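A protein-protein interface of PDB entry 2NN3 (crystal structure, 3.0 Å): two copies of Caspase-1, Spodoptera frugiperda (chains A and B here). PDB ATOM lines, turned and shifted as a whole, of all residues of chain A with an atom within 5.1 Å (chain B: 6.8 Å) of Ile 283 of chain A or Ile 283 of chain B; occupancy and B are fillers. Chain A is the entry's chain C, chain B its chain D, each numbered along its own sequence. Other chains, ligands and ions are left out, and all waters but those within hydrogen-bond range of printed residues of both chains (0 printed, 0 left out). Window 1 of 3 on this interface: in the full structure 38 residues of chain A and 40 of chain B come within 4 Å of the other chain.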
ATOM      1  N   LEU A 211     -10.469 -27.171  10.962  1.00  0.00           N
ATOM      2  CA  LEU A 211     -10.857 -26.275   9.872  1.00  0.00           C
ATOM      3  C   LEU A 211     -12.212 -26.677   9.400  1.00  0.00           C
ATOM      4  O   LEU A 211     -12.459 -27.852   9.177  1.00  0.00           O
ATOM      5  CB  LEU A 211      -9.878 -26.305   8.679  1.00  0.00           C
ATOM      6  CG  LEU A 211     -10.338 -25.583   7.387  1.00  0.00           C
ATOM      7  CD1 LEU A 211     -10.134 -24.109   7.456  1.00  0.00           C
ATOM      8  CD2 LEU A 211      -9.536 -26.079   6.237  1.00  0.00           C
ATOM      9  N   ILE A 212     -13.086 -25.697   9.244  1.00  0.00           N
ATOM     10  CA  ILE A 212     -14.412 -25.939   8.677  1.00  0.00           C
ATOM     11  C   ILE A 212     -14.717 -25.001   7.510  1.00  0.00           C
ATOM     12  O   ILE A 212     -14.819 -23.764   7.706  1.00  0.00           O
ATOM     13  CB  ILE A 212     -15.508 -25.752   9.735  1.00  0.00           C
ATOM     14  CG1 ILE A 212     -15.364 -26.792  10.839  1.00  0.00           C
ATOM     15  CG2 ILE A 212     -16.882 -25.824   9.092  1.00  0.00           C
ATOM     16  CD1 ILE A 212     -15.942 -26.355  12.152  1.00  0.00           C
ATOM     17  N   ALA A 213     -14.874 -25.586   6.316  1.00  0.00           N
ATOM     18  CA  ALA A 213     -15.446 -24.872   5.167  1.00  0.00           C
ATOM     19  C   ALA A 213     -16.893 -25.287   4.946  1.00  0.00           C
ATOM     20  O   ALA A 213     -17.151 -26.403   4.547  1.00  0.00           O
ATOM     21  CB  ALA A 213     -14.649 -25.132   3.944  1.00  0.00           C
ATOM     22  N   LEU A 250      -5.625 -22.132   3.223  1.00  0.00           N
ATOM     23  CA  LEU A 250      -6.491 -20.978   3.407  1.00  0.00           C
ATOM     24  C   LEU A 250      -6.477 -20.023   2.225  1.00  0.00           C
ATOM     25  O   LEU A 250      -7.499 -19.429   1.876  1.00  0.00           O
ATOM     26  CB  LEU A 250      -6.162 -20.257   4.700  1.00  0.00           C
ATOM     27  CG  LEU A 250      -6.634 -20.987   5.953  1.00  0.00           C
ATOM     28  CD1 LEU A 250      -6.185 -20.254   7.195  1.00  0.00           C
ATOM     29  CD2 LEU A 250      -8.121 -21.112   5.935  1.00  0.00           C
ATOM     30  N   LEU A 253      -8.691 -21.825  -0.264  1.00  0.00           N
ATOM     31  CA  LEU A 253     -10.086 -21.745   0.017  1.00  0.00           C
ATOM     32  C   LEU A 253     -10.508 -20.322  -0.248  1.00  0.00           C
ATOM     33  O   LEU A 253     -11.632 -20.078  -0.659  1.00  0.00           O
ATOM     34  CB  LEU A 253     -10.352 -22.180   1.437  1.00  0.00           C
ATOM     35  CG  LEU A 253     -10.346 -23.693   1.663  1.00  0.00           C
ATOM     36  CD1 LEU A 253     -10.542 -23.991   3.118  1.00  0.00           C
ATOM     37  CD2 LEU A 253     -11.444 -24.353   0.876  1.00  0.00           C
ATOM     38  N   CYS A 257     -13.763 -19.351  -2.708  1.00  0.00           N
ATOM     39  CA  CYS A 257     -14.778 -18.331  -2.479  1.00  0.00           C
ATOM     40  C   CYS A 257     -14.949 -17.466  -3.697  1.00  0.00           C
ATOM     41  O   CYS A 257     -16.069 -17.378  -4.221  1.00  0.00           O
ATOM     42  CB  CYS A 257     -14.481 -17.504  -1.241  1.00  0.00           C
ATOM     43  SG  CYS A 257     -14.750 -18.555   0.195  1.00  0.00           S
ATOM     44  N   PRO A 281     -18.971 -19.311   0.381  1.00  0.00           N
ATOM     45  CA  PRO A 281     -18.797 -20.220   1.512  1.00  0.00           C
ATOM     46  C   PRO A 281     -18.227 -19.547   2.786  1.00  0.00           C
ATOM     47  O   PRO A 281     -17.719 -18.445   2.751  1.00  0.00           O
ATOM     48  CB  PRO A 281     -17.801 -21.258   0.992  1.00  0.00           C
ATOM     49  CG  PRO A 281     -17.436 -20.869  -0.351  1.00  0.00           C
ATOM     50  CD  PRO A 281     -17.990 -19.536  -0.680  1.00  0.00           C
ATOM     51  N   CYS A 282     -18.303 -20.231   3.909  1.00  0.00           N
ATOM     52  CA  CYS A 282     -17.779 -19.697   5.137  1.00  0.00           C
ATOM     53  C   CYS A 282     -16.598 -20.489   5.529  1.00  0.00           C
ATOM     54  O   CYS A 282     -16.722 -21.669   5.862  1.00  0.00           O
ATOM     55  CB  CYS A 282     -18.813 -19.806   6.233  1.00  0.00           C
ATOM     56  SG  CYS A 282     -20.173 -18.763   5.813  1.00  0.00           S
ATOM     57  N   ILE A 283     -15.441 -19.854   5.494  1.00  0.00           N
ATOM     58  CA  ILE A 283     -14.256 -20.533   5.970  1.00  0.00           C
ATOM     59  C   ILE A 283     -14.044 -20.168   7.437  1.00  0.00           C
ATOM     60  O   ILE A 283     -13.861 -18.999   7.762  1.00  0.00           O
ATOM     61  CB  ILE A 283     -13.019 -20.193   5.130  1.00  0.00           C
ATOM     62  CG1 ILE A 283     -13.295 -20.348   3.616  1.00  0.00           C
ATOM     63  CG2 ILE A 283     -11.828 -20.990   5.615  1.00  0.00           C
ATOM     64  CD1 ILE A 283     -14.062 -21.572   3.189  1.00  0.00           C
ATOM     65  N   THR A 284     -14.097 -21.165   8.314  1.00  0.00           N
ATOM     66  CA  THR A 284     -13.823 -20.964   9.718  1.00  0.00           C
ATOM     67  C   THR A 284     -12.581 -21.739   9.973  1.00  0.00           C
ATOM     68  O   THR A 284     -12.533 -22.924   9.673  1.00  0.00           O
ATOM     69  CB  THR A 284     -14.934 -21.572  10.559  1.00  0.00           C
ATOM     70  OG1 THR A 284     -16.099 -20.741  10.485  1.00  0.00           O
ATOM     71  CG2 THR A 284     -14.504 -21.701  12.008  1.00  0.00           C
ATOM     72  N   SER A 285     -11.567 -21.102  10.527  1.00  0.00           N
ATOM     73  CA  SER A 285     -10.293 -21.792  10.662  1.00  0.00           C
ATOM     74  C   SER A 285      -9.676 -21.684  12.045  1.00  0.00           C
ATOM     75  O   SER A 285      -9.350 -20.571  12.476  1.00  0.00           O
ATOM     76  CB  SER A 285      -9.313 -21.255   9.625  1.00  0.00           C
ATOM     77  OG  SER A 285      -8.001 -21.645   9.986  1.00  0.00           O
ATOM     78  N   MET A 286      -9.502 -22.808  12.750  1.00  0.00           N
ATOM     79  CA  MET A 286      -8.692 -22.761  13.977  1.00  0.00           C
ATOM     80  C   MET A 286      -7.259 -23.250  13.796  1.00  0.00           C
ATOM     81  O   MET A 286      -6.578 -23.579  14.776  1.00  0.00           O
ATOM     82  CB  MET A 286      -9.320 -23.546  15.104  1.00  0.00           C
ATOM     83  CG  MET A 286     -10.343 -22.787  15.896  1.00  0.00           C
ATOM     84  SD  MET A 286     -11.842 -22.874  14.958  1.00  0.00           S
ATOM     85  CE  MET A 286     -11.988 -21.143  14.621  1.00  0.00           C
ATOM     86  N   TYR B 202     -21.971 -17.449  17.269  1.00  0.00           N
ATOM     87  CA  TYR B 202     -22.716 -16.330  16.670  1.00  0.00           C
ATOM     88  C   TYR B 202     -23.324 -16.624  15.290  1.00  0.00           C
ATOM     89  O   TYR B 202     -23.234 -17.746  14.789  1.00  0.00           O
ATOM     90  CB  TYR B 202     -21.806 -15.100  16.579  1.00  0.00           C
ATOM     91  CG  TYR B 202     -20.580 -15.313  15.722  1.00  0.00           C
ATOM     92  CD1 TYR B 202     -20.574 -14.937  14.388  1.00  0.00           C
ATOM     93  CD2 TYR B 202     -19.428 -15.899  16.246  1.00  0.00           C
ATOM     94  CE1 TYR B 202     -19.453 -15.137  13.586  1.00  0.00           C
ATOM     95  CE2 TYR B 202     -18.302 -16.111  15.457  1.00  0.00           C
ATOM     96  CZ  TYR B 202     -18.319 -15.734  14.119  1.00  0.00           C
ATOM     97  OH  TYR B 202     -17.206 -15.932  13.317  1.00  0.00           O
ATOM     98  N   LEU B 211     -14.784 -10.431   7.367  1.00  0.00           N
ATOM     99  CA  LEU B 211     -13.915 -11.384   8.101  1.00  0.00           C
ATOM    100  C   LEU B 211     -13.969 -11.206   9.603  1.00  0.00           C
ATOM    101  O   LEU B 211     -13.747 -10.113  10.125  1.00  0.00           O
ATOM    102  CB  LEU B 211     -12.457 -11.312   7.638  1.00  0.00           C
ATOM    103  CG  LEU B 211     -11.315 -11.661   8.615  1.00  0.00           C
ATOM    104  CD1 LEU B 211     -10.961 -13.118   8.619  1.00  0.00           C
ATOM    105  CD2 LEU B 211     -10.114 -10.904   8.167  1.00  0.00           C
ATOM    106  N   ILE B 212     -14.229 -12.296  10.306  1.00  0.00           N
ATOM    107  CA  ILE B 212     -14.394 -12.203  11.750  1.00  0.00           C
ATOM    108  C   ILE B 212     -13.358 -12.985  12.558  1.00  0.00           C
ATOM    109  O   ILE B 212     -13.241 -14.206  12.401  1.00  0.00           O
ATOM    110  CB  ILE B 212     -15.798 -12.620  12.165  1.00  0.00           C
ATOM    111  CG1 ILE B 212     -16.822 -11.984  11.211  1.00  0.00           C
ATOM    112  CG2 ILE B 212     -16.028 -12.230  13.598  1.00  0.00           C
ATOM    113  CD1 ILE B 212     -18.231 -12.282  11.520  1.00  0.00           C
ATOM    114  N   ALA B 213     -12.614 -12.272  13.405  1.00  0.00           N
ATOM    115  CA  ALA B 213     -11.587 -12.871  14.271  1.00  0.00           C
ATOM    116  C   ALA B 213     -11.973 -12.712  15.739  1.00  0.00           C
ATOM    117  O   ALA B 213     -11.881 -11.619  16.313  1.00  0.00           O
ATOM    118  CB  ALA B 213     -10.221 -12.235  14.009  1.00  0.00           C
ATOM    119  N   PHE B 214     -12.370 -13.817  16.344  1.00  0.00           N
ATOM    120  CA  PHE B 214     -13.056 -13.807  17.616  1.00  0.00           C
ATOM    121  C   PHE B 214     -12.277 -14.628  18.659  1.00  0.00           C
ATOM    122  O   PHE B 214     -12.031 -15.829  18.452  1.00  0.00           O
ATOM    123  CB  PHE B 214     -14.412 -14.425  17.369  1.00  0.00           C
ATOM    124  CG  PHE B 214     -15.456 -14.023  18.318  1.00  0.00           C
ATOM    125  CD1 PHE B 214     -16.611 -13.414  17.847  1.00  0.00           C
ATOM    126  CD2 PHE B 214     -15.329 -14.286  19.678  1.00  0.00           C
ATOM    127  CE1 PHE B 214     -17.636 -13.039  18.717  1.00  0.00           C
ATOM    128  CE2 PHE B 214     -16.350 -13.911  20.588  1.00  0.00           C
ATOM    129  CZ  PHE B 214     -17.513 -13.290  20.099  1.00  0.00           C
ATOM    130  N   PHE B 232      -4.073 -13.042  23.101  1.00  0.00           N
ATOM    131  CA  PHE B 232      -4.624 -12.760  21.772  1.00  0.00           C
ATOM    132  C   PHE B 232      -4.190 -11.418  21.174  1.00  0.00           C
ATOM    133  O   PHE B 232      -3.609 -11.358  20.099  1.00  0.00           O
ATOM    134  CB  PHE B 232      -6.166 -12.895  21.782  1.00  0.00           C
ATOM    135  CG  PHE B 232      -6.812 -12.566  20.472  1.00  0.00           C
ATOM    136  CD1 PHE B 232      -6.439 -13.220  19.312  1.00  0.00           C
ATOM    137  CD2 PHE B 232      -7.804 -11.600  20.402  1.00  0.00           C
ATOM    138  CE1 PHE B 232      -7.021 -12.902  18.100  1.00  0.00           C
ATOM    139  CE2 PHE B 232      -8.412 -11.284  19.194  1.00  0.00           C
ATOM    140  CZ  PHE B 232      -8.012 -11.925  18.041  1.00  0.00           C
ATOM    141  N   ILE B 249      -3.442 -11.226   5.505  1.00  0.00           N
ATOM    142  CA  ILE B 249      -4.146 -11.173   6.782  1.00  0.00           C
ATOM    143  C   ILE B 249      -4.393 -12.557   7.367  1.00  0.00           C
ATOM    144  O   ILE B 249      -4.339 -12.737   8.575  1.00  0.00           O
ATOM    145  CB  ILE B 249      -5.466 -10.364   6.700  1.00  0.00           C
ATOM    146  CG1 ILE B 249      -6.086 -10.225   8.079  1.00  0.00           C
ATOM    147  CG2 ILE B 249      -6.499 -11.035   5.825  1.00  0.00           C
ATOM    148  CD1 ILE B 249      -5.202  -9.479   9.082  1.00  0.00           C
ATOM    149  N   LEU B 250      -4.645 -13.534   6.508  1.00  0.00           N
ATOM    150  CA  LEU B 250      -4.991 -14.860   6.977  1.00  0.00           C
ATOM    151  C   LEU B 250      -3.814 -15.666   7.507  1.00  0.00           C
ATOM    152  O   LEU B 250      -3.943 -16.373   8.500  1.00  0.00           O
ATOM    153  CB  LEU B 250      -5.714 -15.633   5.895  1.00  0.00           C
ATOM    154  CG  LEU B 250      -7.179 -15.275   5.702  1.00  0.00           C
ATOM    155  CD1 LEU B 250      -7.789 -16.323   4.801  1.00  0.00           C
ATOM    156  CD2 LEU B 250      -7.952 -15.209   7.018  1.00  0.00           C
ATOM    157  N   LEU B 253      -3.153 -14.163  10.855  1.00  0.00           N
ATOM    158  CA  LEU B 253      -3.991 -14.598  11.951  1.00  0.00           C
ATOM    159  C   LEU B 253      -3.709 -16.062  12.249  1.00  0.00           C
ATOM    160  O   LEU B 253      -3.844 -16.499  13.383  1.00  0.00           O
ATOM    161  CB  LEU B 253      -5.456 -14.339  11.662  1.00  0.00           C
ATOM    162  CG  LEU B 253      -5.838 -12.866  11.538  1.00  0.00           C
ATOM    163  CD1 LEU B 253      -7.138 -12.779  10.778  1.00  0.00           C
ATOM    164  CD2 LEU B 253      -5.970 -12.247  12.884  1.00  0.00           C
ATOM    165  N   THR B 254      -3.252 -16.812  11.261  1.00  0.00           N
ATOM    166  CA  THR B 254      -2.849 -18.139  11.583  1.00  0.00           C
ATOM    167  C   THR B 254      -1.771 -18.108  12.656  1.00  0.00           C
ATOM    168  O   THR B 254      -1.922 -18.724  13.701  1.00  0.00           O
ATOM    169  CB  THR B 254      -2.395 -18.882  10.397  1.00  0.00           C
ATOM    170  OG1 THR B 254      -3.502 -19.004   9.496  1.00  0.00           O
ATOM    171  CG2 THR B 254      -1.917 -20.276  10.825  1.00  0.00           C
ATOM    172  N   VAL B 256      -1.165 -15.826  14.745  1.00  0.00           N
ATOM    173  CA  VAL B 256      -1.775 -15.377  15.994  1.00  0.00           C
ATOM    174  C   VAL B 256      -2.340 -16.585  16.785  1.00  0.00           C
ATOM    175  O   VAL B 256      -2.051 -16.760  17.956  1.00  0.00           O
ATOM    176  CB  VAL B 256      -2.871 -14.298  15.745  1.00  0.00           C
ATOM    177  CG1 VAL B 256      -3.758 -14.118  16.969  1.00  0.00           C
ATOM    178  CG2 VAL B 256      -2.255 -12.956  15.343  1.00  0.00           C
ATOM    179  N   CYS B 257      -3.122 -17.433  16.143  1.00  0.00           N
ATOM    180  CA  CYS B 257      -3.548 -18.675  16.779  1.00  0.00           C
ATOM    181  C   CYS B 257      -2.424 -19.460  17.426  1.00  0.00           C
ATOM    182  O   CYS B 257      -2.523 -19.794  18.601  1.00  0.00           O
ATOM    183  CB  CYS B 257      -4.325 -19.540  15.801  1.00  0.00           C
ATOM    184  SG  CYS B 257      -5.773 -18.605  15.237  1.00  0.00           S
ATOM    185  N   PRO B 281      -8.120 -18.478  19.096  1.00  0.00           N
ATOM    186  CA  PRO B 281      -9.113 -17.596  18.432  1.00  0.00           C
ATOM    187  C   PRO B 281      -9.930 -18.307  17.339  1.00  0.00           C
ATOM    188  O   PRO B 281      -9.591 -19.395  16.956  1.00  0.00           O
ATOM    189  CB  PRO B 281      -8.241 -16.504  17.807  1.00  0.00           C
ATOM    190  CG  PRO B 281      -7.019 -16.517  18.597  1.00  0.00           C
ATOM    191  CD  PRO B 281      -6.762 -17.947  18.944  1.00  0.00           C
ATOM    192  N   CYS B 282     -11.005 -17.706  16.854  1.00  0.00           N
ATOM    193  CA  CYS B 282     -11.783 -18.311  15.752  1.00  0.00           C
ATOM    194  C   CYS B 282     -11.759 -17.428  14.560  1.00  0.00           C
ATOM    195  O   CYS B 282     -12.215 -16.304  14.635  1.00  0.00           O
ATOM    196  CB  CYS B 282     -13.243 -18.504  16.132  1.00  0.00           C
ATOM    197  SG  CYS B 282     -13.404 -19.814  17.346  1.00  0.00           S
ATOM    198  N   ILE B 283     -11.239 -17.899  13.446  1.00  0.00           N
ATOM    199  CA  ILE B 283     -11.127 -16.976  12.334  1.00  0.00           C
ATOM    200  C   ILE B 283     -12.131 -17.341  11.288  1.00  0.00           C
ATOM    201  O   ILE B 283     -11.944 -18.345  10.618  1.00  0.00           O
ATOM    202  CB  ILE B 283      -9.734 -16.975  11.696  1.00  0.00           C
ATOM    203  CG1 ILE B 283      -8.629 -17.227  12.742  1.00  0.00           C
ATOM    204  CG2 ILE B 283      -9.530 -15.653  10.972  1.00  0.00           C
ATOM    205  CD1 ILE B 283      -8.470 -16.114  13.780  1.00  0.00           C
ATOM    206  N   THR B 284     -13.198 -16.557  11.153  1.00  0.00           N
ATOM    207  CA  THR B 284     -14.161 -16.833  10.104  1.00  0.00           C
ATOM    208  C   THR B 284     -13.898 -15.915   8.936  1.00  0.00           C
ATOM    209  O   THR B 284     -13.795 -14.709   9.107  1.00  0.00           O
ATOM    210  CB  THR B 284     -15.611 -16.727  10.601  1.00  0.00           C
ATOM    211  OG1 THR B 284     -15.777 -17.608  11.706  1.00  0.00           O
ATOM    212  CG2 THR B 284     -16.598 -17.182   9.568  1.00  0.00           C
ATOM    213  N   SER B 285     -13.770 -16.491   7.749  1.00  0.00           N
ATOM    214  CA  SER B 285     -13.474 -15.709   6.571  1.00  0.00           C
ATOM    215  C   SER B 285     -14.388 -15.952   5.380  1.00  0.00           C
ATOM    216  O   SER B 285     -14.520 -17.082   4.909  1.00  0.00           O
ATOM    217  CB  SER B 285     -12.064 -15.963   6.123  1.00  0.00           C
ATOM    218  OG  SER B 285     -11.787 -15.078   5.071  1.00  0.00           O
ATOM    219  N   MET B 286     -15.001 -14.869   4.907  1.00  0.00           N
ATOM    220  CA  MET B 286     -15.695 -14.845   3.650  1.00  0.00           C
ATOM    221  C   MET B 286     -14.962 -13.950   2.665  1.00  0.00           C
ATOM    222  O   MET B 286     -15.568 -13.451   1.720  1.00  0.00           O
ATOM    223  CB  MET B 286     -17.097 -14.304   3.834  1.00  0.00           C
ATOM    224  CG  MET B 286     -18.130 -15.285   4.322  1.00  0.00           C
ATOM    225  SD  MET B 286     -18.150 -15.353   6.097  1.00  0.00           S
ATOM    226  CE  MET B 286     -17.473 -16.970   6.333  1.00  0.00           C
ATOM    227  N   LEU B 287     -13.667 -13.729   2.889  1.00  0.00           N
ATOM    228  CA  LEU B 287     -12.830 -12.961   1.953  1.00  0.00           C
ATOM    229  C   LEU B 287     -12.712 -13.642   0.576  1.00  0.00           C
ATOM    230  O   LEU B 287     -12.637 -14.886   0.494  1.00  0.00           O
ATOM    231  CB  LEU B 287     -11.436 -12.752   2.528  1.00  0.00           C
ATOM    232  CG  LEU B 287     -11.335 -12.016   3.846  1.00  0.00           C
ATOM    233  CD1 LEU B 287      -9.908 -11.636   4.075  1.00  0.00           C
ATOM    234  CD2 LEU B 287     -12.207 -10.758   3.868  1.00  0.00           C
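O of Ile 283 of chain A is in hydrogen-bond range of N of Ser 285 of chain B. The side-chain hydroxyl (OG1) of Thr 284 of chain A lies within hydrogen-bond range of the side-chain hydroxyl (OG1) of Thr 284 of chain B, at 3.4 Å. The backbone carbonyl oxygen (O) of Ile 283 of chain B is in hydrogen-bond range of the backbone NH (N) of Ser 285 of chain A, 2.8 Å away.
O of Ile 212 of chain A lies within hydrogen-bond range of N of Thr 284 of chain A (2.8 Å). The side-chain sulfur (SG) of Cys 257 of chain A sits at hydrogen-bond distance from the backbone carbonyl oxygen (O) of Leu 253 of chain A, 3.6 Å away. The side-chain hydroxyl of Tyr 202 of chain B sits at hydrogen-bond distance from the side-chain hydroxyl of Thr 284 of chain B, at 2.7 Å. The backbone carbonyl oxygen of Phe 214 of chain B is in hydrogen-bond range of the backbone NH of Cys 282 of chain B (2.7 Å). OG1 of Thr 254 of chain B sits at hydrogen-bond distance from O of Leu 250 of chain B, 2.8 Å away. N of Leu 287 of chain B lies within hydrogen-bond range of OG of Ser 285 of chain B (3.2 Å).
Among the printed residues, pairs that only touch across the chains: Cys 282 of chain A with Met 286 of chain B, Met 286 of chain A with Cys 282 of chain B, Ile 283 of chain A with Thr 284 of chain B, Thr 284 of chain A with Ile 283 of chain B, Ile 283 of chain A with Ile 283 of chain B, Met 286 of chain A with Ile 283 of chain B, Pro 281 of chain A with Met 286 of chain B, Ile 283 of chain A with Met 286 of chain B, Met 286 of chain A with Pro 281 of chain B, Cys 257 of chain A with Leu 287 of chain B and Leu 250 of chain A with Thr 254 of chain B.
Of chain B, only Ile 283 (3.5 Å), Thr 284 (3.2 Å), Ser 285 (2.5 Å) and Met 286 (3.6 Å) come within 4 Å of Ile 283 of chain A. Of the printed residues of chain A, Ile 283 of chain B touches Ile 283, Thr 284, Ser 285 and Met 286. Of the printed residues of chain B, Cys 282 of chain A touches Met 286 (3.0 Å). Printed residues of chain A within 4 Å of Thr 284 of chain B: Ile 283 and Thr 284. Of the printed residues of chain B, Met 286 of chain A touches Pro 281, Cys 282 and Ile 283. Of the printed residues of chain B, Pro 281 of chain A touches Met 286. Leu 211 of chain A touches none of the printed residues of chain B.
Of the 12 printed residues of chain A, 8 touch a printed residue of chain B. Printed residues of chain A that touch a printed residue of chain B: Leu 250, Cys 257, Pro 281, Cys 282, Ile 283, Thr 284, Ser 285 and Met 286. Hydrophobic or aromatic side chains of chain A within 4 Å of the printed part of chain B: Leu 250, Ile 283 and Met 286. Of the 19 printed residues of chain B, 8 touch a printed residue of chain A. Among the printed residues, 14 pairs touch across the chains. Among the printed residues, no Asp or Glu carboxylate lies within 4 Å of a Lys or Arg side-chain nitrogen of the other chain.
Pro 281 of chain A touches Met 286 of chain B, and with the chains exchanged Met 286 of chain A touches Pro 281 of chain B. Cys 282 of chain A touches Met 286 of chain B, and with the chains exchanged Met 286 of chain A touches Cys 282 of chain B. Ile 283 of chain B touches its own counterpart, Ile 283 of chain A. Thr 284 of chain A touches its own counterpart, Thr 284 of chain B.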
